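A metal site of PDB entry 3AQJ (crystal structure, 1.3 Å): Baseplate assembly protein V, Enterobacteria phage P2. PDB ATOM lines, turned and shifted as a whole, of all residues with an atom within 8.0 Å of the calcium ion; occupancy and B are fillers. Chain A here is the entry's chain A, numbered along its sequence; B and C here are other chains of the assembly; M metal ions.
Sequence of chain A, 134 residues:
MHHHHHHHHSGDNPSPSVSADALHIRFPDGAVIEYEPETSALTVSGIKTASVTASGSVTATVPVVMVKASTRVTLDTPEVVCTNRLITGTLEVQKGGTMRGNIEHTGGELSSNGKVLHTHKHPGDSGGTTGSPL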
ATOM      1  N   GLY A 124       4.831  16.958  24.310  1.00  0.00           N
ATOM      2  CA  GLY A 124       3.527  17.725  24.191  1.00  0.00           C
ATOM      3  C   GLY A 124       2.384  16.863  23.707  1.00  0.00           C
ATOM      4  O   GLY A 124       2.583  15.672  23.411  1.00  0.00           O
ATOM      5  N   ASP A 125       1.175  17.430  23.584  1.00  0.00           N
ATOM      6  CA  ASP A 125       0.024  16.625  23.182  1.00  0.00           C
ATOM      7  C   ASP A 125      -0.196  16.560  21.681  1.00  0.00           C
ATOM      8  O   ASP A 125      -1.243  16.007  21.233  1.00  0.00           O
ATOM      9  CB  ASP A 125      -1.256  17.111  23.941  1.00  0.00           C
ATOM     10  CG  ASP A 125      -1.799  18.455  23.477  1.00  0.00           C
ATOM     11  OD1 ASP A 125      -1.191  19.055  22.635  1.00  0.00           O
ATOM     12  OD2 ASP A 125      -2.809  18.865  24.037  1.00  0.00           O
ATOM     13  N   SER A 126       0.718  17.057  20.866  1.00  0.00           N
ATOM     14  CA  SER A 126       0.626  16.988  19.384  1.00  0.00           C
ATOM     15  C   SER A 126       1.866  16.272  18.828  1.00  0.00           C
ATOM     16  O   SER A 126       2.207  16.535  17.675  1.00  0.00           O
ATOM     17  CB  SER A 126       0.560  18.352  18.765  1.00  0.00           C
ATOM     18  OG  SER A 126      -0.613  19.050  19.356  1.00  0.00           O
ATOM     19  N   GLY A 127       2.578  15.546  19.679  1.00  0.00           N
ATOM     20  CA  GLY A 127       3.755  14.781  19.182  1.00  0.00           C
ATOM     21  C   GLY A 127       5.032  15.592  19.185  1.00  0.00           C
ATOM     22  O   GLY A 127       6.039  14.998  18.754  1.00  0.00           O
ATOM     23  N   GLY A 128       5.094  16.843  19.652  1.00  0.00           N
ATOM     24  CA  GLY A 128       6.314  17.648  19.808  1.00  0.00           C
ATOM     25  C   GLY A 128       6.733  17.644  21.251  1.00  0.00           C
ATOM     26  O   GLY A 128       6.394  16.691  21.995  1.00  0.00           O
ATOM     27  N   THR A 130       7.209  20.251  24.748  1.00  0.00           N
ATOM     28  CA  THR A 130       6.941  21.566  25.334  1.00  0.00           C
ATOM     29  C   THR A 130       8.220  22.404  25.497  1.00  0.00           C
ATOM     30  O   THR A 130       9.338  21.851  25.396  1.00  0.00           O
ATOM     31  CB  THR A 130       6.262  21.448  26.692  1.00  0.00           C
ATOM     32  OG1 THR A 130       7.248  20.987  27.702  1.00  0.00           O
ATOM     33  CG2 THR A 130       5.084  20.483  26.733  1.00  0.00           C
ATOM     34  N   GLY B 124      -2.289  19.479  27.798  1.00  0.00           N
ATOM     35  CA  GLY B 124      -1.558  20.005  26.708  1.00  0.00           C
ATOM     36  C   GLY B 124      -2.274  21.190  26.042  1.00  0.00           C
ATOM     37  O   GLY B 124      -3.473  21.461  26.321  1.00  0.00           O
ATOM     38  N   ASP B 125      -1.605  21.851  25.149  1.00  0.00           N
ATOM     39  CA  ASP B 125      -2.177  23.087  24.527  1.00  0.00           C
ATOM     40  C   ASP B 125      -3.235  22.833  23.498  1.00  0.00           C
ATOM     41  O   ASP B 125      -3.872  23.779  23.044  1.00  0.00           O
ATOM     42  CB  ASP B 125      -1.091  24.067  24.046  1.00  0.00           C
ATOM     43  CG  ASP B 125      -0.309  23.616  22.827  1.00  0.00           C
ATOM     44  OD1 ASP B 125      -0.580  22.524  22.301  1.00  0.00           O
ATOM     45  OD2 ASP B 125       0.555  24.464  22.421  1.00  0.00           O
ATOM     46  N   SER B 126      -3.459  21.557  23.155  1.00  0.00           N
ATOM     47  CA  SER B 126      -4.508  21.210  22.168  1.00  0.00           C
ATOM     48  C   SER B 126      -5.643  20.447  22.826  1.00  0.00           C
ATOM     49  O   SER B 126      -6.607  20.080  22.097  1.00  0.00           O
ATOM     50  CB  SER B 126      -3.861  20.305  21.076  1.00  0.00           C
ATOM     51  OG  SER B 126      -2.743  20.972  20.443  1.00  0.00           O
ATOM     52  N   GLY B 127      -5.618  20.247  24.111  1.00  0.00           N
ATOM     53  CA  GLY B 127      -6.681  19.564  24.798  1.00  0.00           C
ATOM     54  C   GLY B 127      -6.443  18.125  25.186  1.00  0.00           C
ATOM     55  O   GLY B 127      -7.272  17.482  25.789  1.00  0.00           O
ATOM     56  N   GLY B 128      -5.264  17.609  24.899  1.00  0.00           N
ATOM     57  CA  GLY B 128      -4.816  16.293  25.356  1.00  0.00           C
ATOM     58  C   GLY B 128      -4.014  16.458  26.608  1.00  0.00           C
ATOM     59  O   GLY B 128      -4.194  17.422  27.388  1.00  0.00           O
ATOM     60  N   THR B 130       0.110  16.097  28.263  1.00  0.00           N
ATOM     61  CA  THR B 130       1.543  15.864  28.034  1.00  0.00           C
ATOM     62  C   THR B 130       1.981  14.543  28.577  1.00  0.00           C
ATOM     63  O   THR B 130       1.314  13.882  29.336  1.00  0.00           O
ATOM     64  CB  THR B 130       2.400  17.009  28.682  1.00  0.00           C
ATOM     65  OG1 THR B 130       2.395  16.859  30.080  1.00  0.00           O
ATOM     66  CG2 THR B 130       1.896  18.413  28.308  1.00  0.00           C
ATOM     67  N   GLY C 124       3.381  25.117  25.027  1.00  0.00           N
ATOM     68  CA  GLY C 124       3.036  23.826  24.457  1.00  0.00           C
ATOM     69  C   GLY C 124       3.634  23.582  23.123  1.00  0.00           C
ATOM     70  O   GLY C 124       4.401  24.362  22.621  1.00  0.00           O
ATOM     71  N   ASP C 125       3.294  22.445  22.527  1.00  0.00           N
ATOM     72  CA  ASP C 125       3.902  22.042  21.247  1.00  0.00           C
ATOM     73  C   ASP C 125       3.111  22.543  20.072  1.00  0.00           C
ATOM     74  O   ASP C 125       3.508  22.245  18.922  1.00  0.00           O
ATOM     75  CB  ASP C 125       4.213  20.561  21.133  1.00  0.00           C
ATOM     76  CG  ASP C 125       2.987  19.704  21.084  1.00  0.00           C
ATOM     77  OD1 ASP C 125       1.794  20.196  21.059  1.00  0.00           O
ATOM     78  OD2 ASP C 125       3.142  18.487  21.071  1.00  0.00           O
ATOM     79  N   SER C 126       2.080  23.372  20.219  1.00  0.00           N
ATOM     80  CA  SER C 126       1.343  23.930  19.103  1.00  0.00           C
ATOM     81  C   SER C 126       1.264  25.479  19.125  1.00  0.00           C
ATOM     82  O   SER C 126       0.468  26.071  18.379  1.00  0.00           O
ATOM     83  CB  SER C 126      -0.120  23.441  19.111  1.00  0.00           C
ATOM     84  OG  SER C 126      -0.164  22.048  19.140  1.00  0.00           O
ATOM     85  N   GLY C 127       2.026  26.131  19.985  1.00  0.00           N
ATOM     86  CA  GLY C 127       2.103  27.602  20.084  1.00  0.00           C
ATOM     87  C   GLY C 127       1.208  28.184  21.155  1.00  0.00           C
ATOM     88  O   GLY C 127       1.105  29.415  21.216  1.00  0.00           O
ATOM     89  N   GLY C 128       0.539  27.341  21.946  1.00  0.00           N
ATOM     90  CA  GLY C 128      -0.181  27.909  23.133  1.00  0.00           C
ATOM     91  C   GLY C 128       0.622  27.512  24.349  1.00  0.00           C
ATOM     92  O   GLY C 128       1.840  27.466  24.322  1.00  0.00           O
ATOM     93  N   THR C 129      -0.052  27.330  25.488  1.00  0.00           N
ATOM     94  CA  THR C 129       0.570  26.861  26.736  1.00  0.00           C
ATOM     95  C   THR C 129      -0.124  25.625  27.270  1.00  0.00           C
ATOM     96  O   THR C 129      -1.300  25.377  26.971  1.00  0.00           O
ATOM     97  CB  THR C 129       0.670  27.958  27.818  1.00  0.00           C
ATOM     98  OG1 THR C 129      -0.704  28.306  28.246  1.00  0.00           O
ATOM     99  CG2 THR C 129       1.407  29.181  27.357  1.00  0.00           C
ATOM    100  N   THR C 130       0.595  24.843  28.038  1.00  0.00           N
ATOM    101  CA  THR C 130      -0.020  23.717  28.784  1.00  0.00           C
ATOM    102  C   THR C 130      -0.875  24.348  29.938  1.00  0.00           C
ATOM    103  O   THR C 130      -0.740  25.531  30.253  1.00  0.00           O
ATOM    104  CB  THR C 130       1.057  22.857  29.328  1.00  0.00           C
ATOM    105  OG1 THR C 130       1.788  23.515  30.410  1.00  0.00           O
ATOM    106  CG2 THR C 130       2.085  22.334  28.298  1.00  0.00           C
HETATM  107 CA    CA M   1      -0.405  20.636  21.117  1.00  0.00          CA
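The backbone NH (N) of Gly 127 of chain C sits at hydrogen-bond distance from the side-chain carboxylate (OD2) of Asp 125 of chain B, at 3.3 Å. The backbone NH of Gly 128 of chain C is in hydrogen-bond range of the side-chain carboxylate of Asp 125 of chain B (2.9 Å). OD2 of Asp 125 of chain C is in hydrogen-bond range of N of Gly 127 of chain A (3.3 Å). The side-chain carboxylate (OD2) of Asp 125 of chain C sits at hydrogen-bond distance from the backbone NH (N) of Gly 128 of chain A. The backbone NH (N) of Gly 127 of chain B sits at hydrogen-bond distance from the side-chain carboxylate (OD2) of Asp 125 of chain A (3.1 Å). OD2 of Asp 125 of chain A is in hydrogen-bond range of N of Gly 128 of chain B.
The nearest printed residue that does not touch the calcium ion is Gly 124 of chain B (5.3 Å).
The calcium ion is bound by the side-chain carboxylate (OD1) of Asp 125 of chain B (2.2 Å), the side-chain carboxylate (OD1) of Asp 125 of chain C (2.2 Å), the side-chain carboxylate (OD1) of Asp 125 of chain A (2.3 Å), the side-chain hydroxyl (OG) of Ser 126 of chain A (2.4 Å), the side-chain hydroxyl (OG) of Ser 126 of chain C (2.4 Å) and the side-chain hydroxyl (OG) of Ser 126 of chain B (2.5 Å). The calcium ion has six donor atoms within binding distance.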
